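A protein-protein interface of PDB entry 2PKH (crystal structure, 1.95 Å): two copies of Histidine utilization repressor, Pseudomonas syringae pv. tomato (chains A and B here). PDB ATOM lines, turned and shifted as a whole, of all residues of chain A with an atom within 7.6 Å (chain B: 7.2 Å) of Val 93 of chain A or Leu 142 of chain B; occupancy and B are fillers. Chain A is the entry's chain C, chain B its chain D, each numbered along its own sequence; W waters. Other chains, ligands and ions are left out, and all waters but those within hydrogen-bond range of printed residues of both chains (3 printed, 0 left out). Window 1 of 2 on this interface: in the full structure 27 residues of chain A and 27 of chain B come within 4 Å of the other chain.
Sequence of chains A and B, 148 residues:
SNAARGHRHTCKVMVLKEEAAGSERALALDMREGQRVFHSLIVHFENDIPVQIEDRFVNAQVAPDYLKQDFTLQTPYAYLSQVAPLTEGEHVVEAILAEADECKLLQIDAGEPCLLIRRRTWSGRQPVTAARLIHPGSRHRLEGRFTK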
ATOM      1  N   HIS A  91       5.705 -10.868  25.359  1.00  0.00           N
ATOM      2  CA  HIS A  91       4.788 -11.789  24.676  1.00  0.00           C
ATOM      3  C   HIS A  91       5.556 -12.764  23.821  1.00  0.00           C
ATOM      4  O   HIS A  91       6.616 -12.448  23.302  1.00  0.00           O
ATOM      5  CB  HIS A  91       3.776 -11.021  23.878  1.00  0.00           C
ATOM      6  CG  HIS A  91       4.383 -10.132  22.833  1.00  0.00           C
ATOM      7  ND1 HIS A  91       4.963 -10.624  21.675  1.00  0.00           N
ATOM      8  CD2 HIS A  91       4.496  -8.784  22.765  1.00  0.00           C
ATOM      9  CE1 HIS A  91       5.395  -9.621  20.929  1.00  0.00           C
ATOM     10  NE2 HIS A  91       5.109  -8.489  21.562  1.00  0.00           N
ATOM     11  N   VAL A  92       5.072 -13.983  23.696  1.00  0.00           N
ATOM     12  CA  VAL A  92       5.662 -14.953  22.754  1.00  0.00           C
ATOM     13  C   VAL A  92       4.436 -15.510  22.009  1.00  0.00           C
ATOM     14  O   VAL A  92       3.464 -15.914  22.666  1.00  0.00           O
ATOM     15  CB  VAL A  92       6.405 -16.088  23.462  1.00  0.00           C
ATOM     16  CG1 VAL A  92       6.659 -17.236  22.518  1.00  0.00           C
ATOM     17  CG2 VAL A  92       7.655 -15.624  24.059  1.00  0.00           C
ATOM     18  N   VAL A  93       4.465 -15.510  20.678  1.00  0.00           N
ATOM     19  CA  VAL A  93       3.328 -15.952  19.884  1.00  0.00           C
ATOM     20  C   VAL A  93       3.747 -17.159  19.144  1.00  0.00           C
ATOM     21  O   VAL A  93       4.751 -17.110  18.429  1.00  0.00           O
ATOM     22  CB  VAL A  93       2.903 -14.823  18.868  1.00  0.00           C
ATOM     23  CG1 VAL A  93       1.692 -15.250  17.938  1.00  0.00           C
ATOM     24  CG2 VAL A  93       2.662 -13.469  19.568  1.00  0.00           C
ATOM     25  N   GLU A  94       2.990 -18.267  19.299  1.00  0.00           N
ATOM     26  CA  GLU A  94       3.317 -19.524  18.613  1.00  0.00           C
ATOM     27  C   GLU A  94       2.059 -20.059  18.005  1.00  0.00           C
ATOM     28  O   GLU A  94       0.939 -19.710  18.476  1.00  0.00           O
ATOM     29  CB  GLU A  94       3.829 -20.565  19.684  1.00  0.00           C
ATOM     30  CG  GLU A  94       5.272 -20.309  20.020  1.00  0.00           C
ATOM     31  CD  GLU A  94       5.846 -21.358  20.985  1.00  0.00           C
ATOM     32  OE1 GLU A  94       5.795 -22.591  20.758  1.00  0.00           O
ATOM     33  OE2 GLU A  94       6.335 -20.902  22.009  1.00  0.00           O
ATOM     34  N   ALA A  95       2.245 -20.909  16.997  1.00  0.00           N
ATOM     35  CA  ALA A  95       1.152 -21.704  16.444  1.00  0.00           C
ATOM     36  C   ALA A  95       1.319 -23.102  17.021  1.00  0.00           C
ATOM     37  O   ALA A  95       2.361 -23.752  16.802  1.00  0.00           O
ATOM     38  CB  ALA A  95       1.229 -21.756  14.940  1.00  0.00           C
ATOM     39  N   ILE A  96       0.299 -23.554  17.739  1.00  0.00           N
ATOM     40  CA  ILE A  96       0.344 -24.851  18.435  1.00  0.00           C
ATOM     41  C   ILE A  96      -0.899 -25.670  18.230  1.00  0.00           C
ATOM     42  O   ILE A  96      -1.909 -25.155  17.787  1.00  0.00           O
ATOM     43  CB  ILE A  96       0.477 -24.619  19.933  1.00  0.00           C
ATOM     44  CG1 ILE A  96      -0.777 -23.939  20.539  1.00  0.00           C
ATOM     45  CG2 ILE A  96       1.759 -23.735  20.255  1.00  0.00           C
ATOM     46  CD1 ILE A  96      -0.849 -23.993  22.122  1.00  0.00           C
ATOM     47  N   CYS A 114      -4.002 -23.468  16.831  1.00  0.00           N
ATOM     48  CA  CYS A 114      -4.423 -22.383  17.694  1.00  0.00           C
ATOM     49  C   CYS A 114      -3.301 -21.360  17.766  1.00  0.00           C
ATOM     50  O   CYS A 114      -2.144 -21.725  17.610  1.00  0.00           O
ATOM     51  CB  CYS A 114      -4.635 -22.939  19.124  1.00  0.00           C
ATOM     52  SG  CYS A 114      -6.109 -23.928  19.260  1.00  0.00           S
ATOM     53  N   LEU A 115      -3.655 -20.081  17.971  1.00  0.00           N
ATOM     54  CA  LEU A 115      -2.629 -19.048  18.187  1.00  0.00           C
ATOM     55  C   LEU A 115      -2.452 -18.995  19.660  1.00  0.00           C
ATOM     56  O   LEU A 115      -3.434 -18.822  20.359  1.00  0.00           O
ATOM     57  CB  LEU A 115      -3.163 -17.692  17.723  1.00  0.00           C
ATOM     58  CG  LEU A 115      -2.620 -16.999  16.498  1.00  0.00           C
ATOM     59  CD1 LEU A 115      -3.139 -15.566  16.665  1.00  0.00           C
ATOM     60  CD2 LEU A 115      -1.098 -17.089  16.386  1.00  0.00           C
ATOM     61  N   LEU A 116      -1.233 -19.193  20.152  1.00  0.00           N
ATOM     62  CA  LEU A 116      -0.937 -19.044  21.546  1.00  0.00           C
ATOM     63  C   LEU A 116      -0.170 -17.750  21.725  1.00  0.00           C
ATOM     64  O   LEU A 116       0.741 -17.450  20.980  1.00  0.00           O
ATOM     65  CB  LEU A 116       0.012 -20.175  21.966  1.00  0.00           C
ATOM     66  CG  LEU A 116       0.792 -19.948  23.305  1.00  0.00           C
ATOM     67  CD1 LEU A 116      -0.181 -20.177  24.468  1.00  0.00           C
ATOM     68  CD2 LEU A 116       1.985 -20.832  23.406  1.00  0.00           C
ATOM     69  N   ILE A 117      -0.561 -16.929  22.670  1.00  0.00           N
ATOM     70  CA  ILE A 117       0.229 -15.781  23.079  1.00  0.00           C
ATOM     71  C   ILE A 117       0.571 -16.005  24.557  1.00  0.00           C
ATOM     72  O   ILE A 117      -0.333 -16.058  25.444  1.00  0.00           O
ATOM     73  CB  ILE A 117      -0.579 -14.509  23.031  1.00  0.00           C
ATOM     74  CG1 ILE A 117      -1.049 -14.242  21.581  1.00  0.00           C
ATOM     75  CG2 ILE A 117       0.282 -13.391  23.538  1.00  0.00           C
ATOM     76  CD1 ILE A 117      -2.110 -13.109  21.501  1.00  0.00           C
ATOM     77  N   ARG A 118       1.837 -16.212  24.856  1.00  0.00           N
ATOM     78  CA  ARG A 118       2.260 -16.359  26.274  1.00  0.00           C
ATOM     79  C   ARG A 118       2.672 -14.971  26.720  1.00  0.00           C
ATOM     80  O   ARG A 118       3.478 -14.319  26.015  1.00  0.00           O
ATOM     81  CB  ARG A 118       3.499 -17.167  26.364  1.00  0.00           C
ATOM     82  CG  ARG A 118       3.289 -18.597  26.142  1.00  0.00           C
ATOM     83  CD  ARG A 118       4.247 -19.452  26.996  1.00  0.00           C
ATOM     84  NE  ARG A 118       5.671 -19.172  26.767  1.00  0.00           N
ATOM     85  CZ  ARG A 118       6.401 -19.677  25.767  1.00  0.00           C
ATOM     86  NH1 ARG A 118       5.824 -20.475  24.832  1.00  0.00           N
ATOM     87  NH2 ARG A 118       7.681 -19.331  25.656  1.00  0.00           N
ATOM     88  N   ARG A 119       2.187 -14.532  27.873  1.00  0.00           N
ATOM     89  CA  ARG A 119       2.428 -13.169  28.311  1.00  0.00           C
ATOM     90  C   ARG A 119       3.054 -13.218  29.693  1.00  0.00           C
ATOM     91  O   ARG A 119       2.635 -14.016  30.536  1.00  0.00           O
ATOM     92  CB  ARG A 119       1.110 -12.394  28.411  1.00  0.00           C
ATOM     93  CG  ARG A 119       0.378 -12.077  27.055  1.00  0.00           C
ATOM     94  CD  ARG A 119      -0.310 -10.673  27.020  1.00  0.00           C
ATOM     95  NE  ARG A 119      -0.514 -10.301  25.610  1.00  0.00           N
ATOM     96  CZ  ARG A 119       0.280  -9.521  24.864  1.00  0.00           C
ATOM     97  NH1 ARG A 119       1.345  -8.889  25.375  1.00  0.00           N
ATOM     98  NH2 ARG A 119      -0.028  -9.339  23.576  1.00  0.00           N
ATOM     99  N   LEU A 142      -4.246 -11.936  14.785  1.00  0.00           N
ATOM    100  CA  LEU A 142      -3.678 -10.722  15.341  1.00  0.00           C
ATOM    101  C   LEU A 142      -3.550  -9.791  14.149  1.00  0.00           C
ATOM    102  O   LEU A 142      -3.112 -10.240  13.084  1.00  0.00           O
ATOM    103  CB  LEU A 142      -2.286 -10.968  15.935  1.00  0.00           C
ATOM    104  CG  LEU A 142      -2.156 -11.994  17.057  1.00  0.00           C
ATOM    105  CD1 LEU A 142      -0.644 -12.133  17.478  1.00  0.00           C
ATOM    106  CD2 LEU A 142      -3.127 -11.683  18.198  1.00  0.00           C
ATOM    107  N   VAL B  93      -1.412 -12.008  11.711  1.00  0.00           N
ATOM    108  CA  VAL B  93      -0.782 -13.255  12.142  1.00  0.00           C
ATOM    109  C   VAL B  93      -1.902 -14.273  12.483  1.00  0.00           C
ATOM    110  O   VAL B  93      -2.870 -13.948  13.200  1.00  0.00           O
ATOM    111  CB  VAL B  93       0.131 -13.006  13.406  1.00  0.00           C
ATOM    112  CG1 VAL B  93       0.838 -14.310  13.853  1.00  0.00           C
ATOM    113  CG2 VAL B  93       1.146 -11.893  13.163  1.00  0.00           C
ATOM    114  N   GLU B  94      -1.760 -15.496  11.974  1.00  0.00           N
ATOM    115  CA  GLU B  94      -2.751 -16.525  12.151  1.00  0.00           C
ATOM    116  C   GLU B  94      -2.073 -17.856  12.361  1.00  0.00           C
ATOM    117  O   GLU B  94      -0.933 -18.022  11.943  1.00  0.00           O
ATOM    118  CB  GLU B  94      -3.541 -16.663  10.872  1.00  0.00           C
ATOM    119  CG  GLU B  94      -4.493 -15.559  10.645  1.00  0.00           C
ATOM    120  CD  GLU B  94      -4.997 -15.613   9.216  1.00  0.00           C
ATOM    121  OE1 GLU B  94      -5.783 -16.534   8.893  1.00  0.00           O
ATOM    122  OE2 GLU B  94      -4.567 -14.795   8.401  1.00  0.00           O
ATOM    123  N   LEU B 115       2.684 -20.720  11.809  1.00  0.00           N
ATOM    124  CA  LEU B 115       2.402 -19.274  11.942  1.00  0.00           C
ATOM    125  C   LEU B 115       2.316 -18.697  10.580  1.00  0.00           C
ATOM    126  O   LEU B 115       3.283 -18.802   9.867  1.00  0.00           O
ATOM    127  CB  LEU B 115       3.555 -18.485  12.620  1.00  0.00           C
ATOM    128  CG  LEU B 115       3.459 -18.182  14.114  1.00  0.00           C
ATOM    129  CD1 LEU B 115       4.618 -17.256  14.665  1.00  0.00           C
ATOM    130  CD2 LEU B 115       2.088 -17.696  14.528  1.00  0.00           C
ATOM    131  N   LEU B 116       1.167 -18.142  10.187  1.00  0.00           N
ATOM    132  CA  LEU B 116       1.059 -17.428   8.907  1.00  0.00           C
ATOM    133  C   LEU B 116       1.204 -15.931   9.229  1.00  0.00           C
ATOM    134  O   LEU B 116       0.549 -15.444  10.174  1.00  0.00           O
ATOM    135  CB  LEU B 116      -0.314 -17.729   8.272  1.00  0.00           C
ATOM    136  CG  LEU B 116      -0.689 -16.870   7.059  1.00  0.00           C
ATOM    137  CD1 LEU B 116       0.351 -17.084   5.959  1.00  0.00           C
ATOM    138  CD2 LEU B 116      -2.130 -17.099   6.588  1.00  0.00           C
ATOM    139  N   ILE B 117       2.109 -15.221   8.537  1.00  0.00           N
ATOM    140  CA  ILE B 117       2.194 -13.758   8.639  1.00  0.00           C
ATOM    141  C   ILE B 117       1.953 -13.218   7.248  1.00  0.00           C
ATOM    142  O   ILE B 117       2.640 -13.601   6.310  1.00  0.00           O
ATOM    143  CB  ILE B 117       3.547 -13.230   9.211  1.00  0.00           C
ATOM    144  CG1 ILE B 117       3.851 -13.915  10.564  1.00  0.00           C
ATOM    145  CG2 ILE B 117       3.473 -11.688   9.298  1.00  0.00           C
ATOM    146  CD1 ILE B 117       5.201 -13.610  11.131  1.00  0.00           C
ATOM    147  N   ARG B 119       1.642  -9.805   5.147  1.00  0.00           N
ATOM    148  CA  ARG B 119       2.128  -8.451   5.277  1.00  0.00           C
ATOM    149  C   ARG B 119       1.814  -7.715   4.012  1.00  0.00           C
ATOM    150  O   ARG B 119       1.771  -8.318   2.918  1.00  0.00           O
ATOM    151  CB  ARG B 119       3.641  -8.435   5.493  1.00  0.00           C
ATOM    152  CG  ARG B 119       4.082  -9.013   6.812  1.00  0.00           C
ATOM    153  CD  ARG B 119       5.501  -8.525   7.188  1.00  0.00           C
ATOM    154  NE  ARG B 119       5.799  -8.864   8.591  1.00  0.00           N
ATOM    155  CZ  ARG B 119       6.991  -9.229   9.049  1.00  0.00           C
ATOM    156  NH1 ARG B 119       8.051  -9.321   8.225  1.00  0.00           N
ATOM    157  NH2 ARG B 119       7.106  -9.540  10.334  1.00  0.00           N
ATOM    158  N   HIS B 135       5.654 -20.224   8.571  1.00  0.00           N
ATOM    159  CA  HIS B 135       6.730 -20.795   9.417  1.00  0.00           C
ATOM    160  C   HIS B 135       6.148 -22.025  10.102  1.00  0.00           C
ATOM    161  O   HIS B 135       5.069 -21.918  10.644  1.00  0.00           O
ATOM    162  CB  HIS B 135       7.129 -19.812  10.540  1.00  0.00           C
ATOM    163  CG  HIS B 135       7.469 -18.423  10.079  1.00  0.00           C
ATOM    164  ND1 HIS B 135       6.505 -17.448   9.881  1.00  0.00           N
ATOM    165  CD2 HIS B 135       8.663 -17.832   9.803  1.00  0.00           C
ATOM    166  CE1 HIS B 135       7.087 -16.312   9.514  1.00  0.00           C
ATOM    167  NE2 HIS B 135       8.394 -16.511   9.481  1.00  0.00           N
ATOM    168  N   GLY B 137       5.191 -24.190  13.093  1.00  0.00           N
ATOM    169  CA  GLY B 137       4.977 -23.805  14.488  1.00  0.00           C
ATOM    170  C   GLY B 137       6.079 -24.254  15.449  1.00  0.00           C
ATOM    171  O   GLY B 137       6.356 -23.593  16.445  1.00  0.00           O
ATOM    172  N   HIS B 140       9.496 -21.646  14.667  1.00  0.00           N
ATOM    173  CA  HIS B 140       9.629 -20.169  14.801  1.00  0.00           C
ATOM    174  C   HIS B 140       8.661 -19.683  15.858  1.00  0.00           C
ATOM    175  O   HIS B 140       7.610 -20.307  16.069  1.00  0.00           O
ATOM    176  CB  HIS B 140       9.174 -19.600  13.519  1.00  0.00           C
ATOM    177  CG  HIS B 140       9.419 -18.142  13.361  1.00  0.00           C
ATOM    178  ND1 HIS B 140      10.673 -17.591  13.461  1.00  0.00           N
ATOM    179  CD2 HIS B 140       8.582 -17.133  13.047  1.00  0.00           C
ATOM    180  CE1 HIS B 140      10.597 -16.296  13.261  1.00  0.00           C
ATOM    181  NE2 HIS B 140       9.341 -15.995  12.995  1.00  0.00           N
ATOM    182  N   ARG B 141       8.957 -18.572  16.517  1.00  0.00           N
ATOM    183  CA  ARG B 141       7.918 -17.857  17.277  1.00  0.00           C
ATOM    184  C   ARG B 141       8.251 -16.390  17.186  1.00  0.00           C
ATOM    185  O   ARG B 141       9.380 -16.061  16.787  1.00  0.00           O
ATOM    186  CB  ARG B 141       7.938 -18.281  18.734  1.00  0.00           C
ATOM    187  CG  ARG B 141       9.394 -18.219  19.377  1.00  0.00           C
ATOM    188  CD  ARG B 141       9.368 -18.727  20.845  1.00  0.00           C
ATOM    189  NE  ARG B 141      10.718 -18.580  21.331  1.00  0.00           N
ATOM    190  CZ  ARG B 141      11.173 -18.936  22.528  1.00  0.00           C
ATOM    191  NH1 ARG B 141      10.374 -19.479  23.447  1.00  0.00           N
ATOM    192  NH2 ARG B 141      12.448 -18.727  22.795  1.00  0.00           N
ATOM    193  N   LEU B 142       7.280 -15.533  17.516  1.00  0.00           N
ATOM    194  CA  LEU B 142       7.442 -14.059  17.554  1.00  0.00           C
ATOM    195  C   LEU B 142       7.634 -13.736  18.989  1.00  0.00           C
ATOM    196  O   LEU B 142       6.863 -14.192  19.784  1.00  0.00           O
ATOM    197  CB  LEU B 142       6.186 -13.309  17.109  1.00  0.00           C
ATOM    198  CG  LEU B 142       5.750 -13.137  15.646  1.00  0.00           C
ATOM    199  CD1 LEU B 142       6.280 -14.214  14.774  1.00  0.00           C
ATOM    200  CD2 LEU B 142       4.256 -12.987  15.478  1.00  0.00           C
ATOM    201  N   GLU B 143       8.628 -12.922  19.333  1.00  0.00           N
ATOM    202  CA  GLU B 143       8.901 -12.646  20.746  1.00  0.00           C
ATOM    203  C   GLU B 143       9.053 -11.159  20.895  1.00  0.00           C
ATOM    204  O   GLU B 143       9.647 -10.527  20.041  1.00  0.00           O
ATOM    205  CB  GLU B 143      10.219 -13.270  21.153  1.00  0.00           C
ATOM    206  CG  GLU B 143      10.199 -14.751  21.350  1.00  0.00           C
ATOM    207  CD  GLU B 143      11.601 -15.335  21.245  1.00  0.00           C
ATOM    208  OE1 GLU B 143      12.595 -14.614  21.475  1.00  0.00           O
ATOM    209  OE2 GLU B 143      11.718 -16.506  20.910  1.00  0.00           O
ATOM    210  N   GLY B 144       8.563 -10.595  21.988  1.00  0.00           N
ATOM    211  CA  GLY B 144       8.780  -9.160  22.234  1.00  0.00           C
ATOM    212  C   GLY B 144       8.748  -8.902  23.716  1.00  0.00           C
ATOM    213  O   GLY B 144       8.037  -9.617  24.444  1.00  0.00           O
HETATM  214  O   HOH W   1       5.487 -24.357  19.017  1.00  0.00           O
HETATM  215  O   HOH W   2       5.204 -20.996  16.231  1.00  0.00           O
HETATM  216  O   HOH W   3       8.496 -20.973  23.053  1.00  0.00           O
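N of His 91 of chain A lies within hydrogen-bond range of O of Gly 144 of chain B (2.8 Å).
The backbone NH (N) of Val 93 of chain A sits at hydrogen-bond distance from the backbone carbonyl oxygen (O) of Leu 142 of chain B, 2.9 Å away.
The backbone NH (N) of Val 93 of chain B is in hydrogen-bond range of the backbone carbonyl oxygen (O) of Leu 142 of chain A (2.8 Å).
The guanidinium group (NH1) of Arg 141 of chain B sits close to the guanidinium group (NH2) of Arg 118 of chain A.
O of Val 92 of chain A sits at hydrogen-bond distance from N of Arg 118 of chain A (2.7 Å).
O of Glu 94 of chain A lies within hydrogen-bond range of N of Leu 116 of chain A (2.8 Å).
OE2 of Glu 94 of chain A is in salt-bridge range of NH1 of Arg 118 of chain A (2.9 Å).
The backbone carbonyl oxygen of His 135 of chain B sits at hydrogen-bond distance from the backbone NH of Leu 115 of chain B, 2.9 Å away.
NH2 of Arg 141 of chain B lies within salt-bridge range of OE2 of Glu 143 of chain B (3.0 Å).
Val 93 of chain A touches just these residues of chain B: Leu 115 (3.8 Å), Arg 141 (3.4 Å) and Leu 142 (2.9 Å).
Printed residues of chain B within 4 Å of Arg 118 of chain A: Arg 141 (3.5 Å).
Printed residues of chain A within 4 Å of Val 93 of chain B: Leu 115 and Leu 142.
Of the printed residues of chain A, Arg 141 of chain B touches Val 92 (3.5 Å), Val 93 (3.4 Å), Glu 94 (3.6 Å) and Arg 118 (3.5 Å).
Printed residues of chain B within 4 Å of Ala 95 of chain A: Leu 115 (3.6 Å) and Gly 137 (3.5 Å).
Ile 117 of chain B touches none of the printed residues of chain A.
Leu 116 of chain B touches none of the printed residues of chain A.
Of the 13 printed residues of chain A, 8 touch a printed residue of chain B.
Among the printed residues, no Asp or Glu carboxylate lies within 4 Å of a Lys or Arg side-chain nitrogen of the other chain.
Water W3 lies within hydrogen-bond range of the side-chain carboxylate (OE2) of Glu 94 of chain A (2.4 Å), the guanidinium group (NH1) of Arg 141 of chain B (2.4 Å) and the guanidinium group (NH2) of Arg 118 of chain A (3.2 Å).
Water W1 lies within hydrogen-bond range of the side-chain carboxylate of Glu 94 of chain A (2.5 Å) and the backbone carbonyl oxygen of Gly 137 of chain B (2.8 Å).
Water W2 lies within hydrogen-bond range of the backbone carbonyl oxygen of His 140 of chain B, the backbone carbonyl oxygen of Gly 137 of chain B and the backbone NH of Ala 95 of chain A.
Leu 142 of chain B touches His 91 of chain A.
CG1 of Val 92 of chain A touches CD of Arg 141 of chain B (3.5 Å).
Leu 142 of chain B touches Val 92 of chain A.
CG of Glu 143 of chain B touches CG2 of Val 92 of chain A, at 3.8 Å.
CD1 of Leu 115 of chain B touches O of Val 93 of chain A, 3.8 Å away.
O of Val 93 of chain A touches CB of Arg 141 of chain B, 3.4 Å away.
CG of Glu 94 of chain A touches CB of Arg 141 of chain B, at 3.6 Å.
Leu 115 of chain B touches Ala 95 of chain A.
Gly 137 of chain B touches Ala 95 of chain A (CA to O, 3.5 Å).
O of Val 93 of chain B touches CD1 of Leu 115 of chain A, 3.8 Å away.
Val 93 of chain A touches Leu 115 of chain B, and with the chains exchanged Leu 115 of chain A touches Val 93 of chain B.
Val 93 of chain A touches Leu 142 of chain B, and with the chains exchanged Leu 142 of chain A touches Val 93 of chain B.
Leu 115 of chain B touches its own counterpart, Leu 115 of chain A.
Positions printed for both chains: 93, 94, 115, 116, 117, 119 and 142.
Of the 16 pairs that touch across the chains among the printed residues, 5 have their exchanged pair printed and touching as well.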
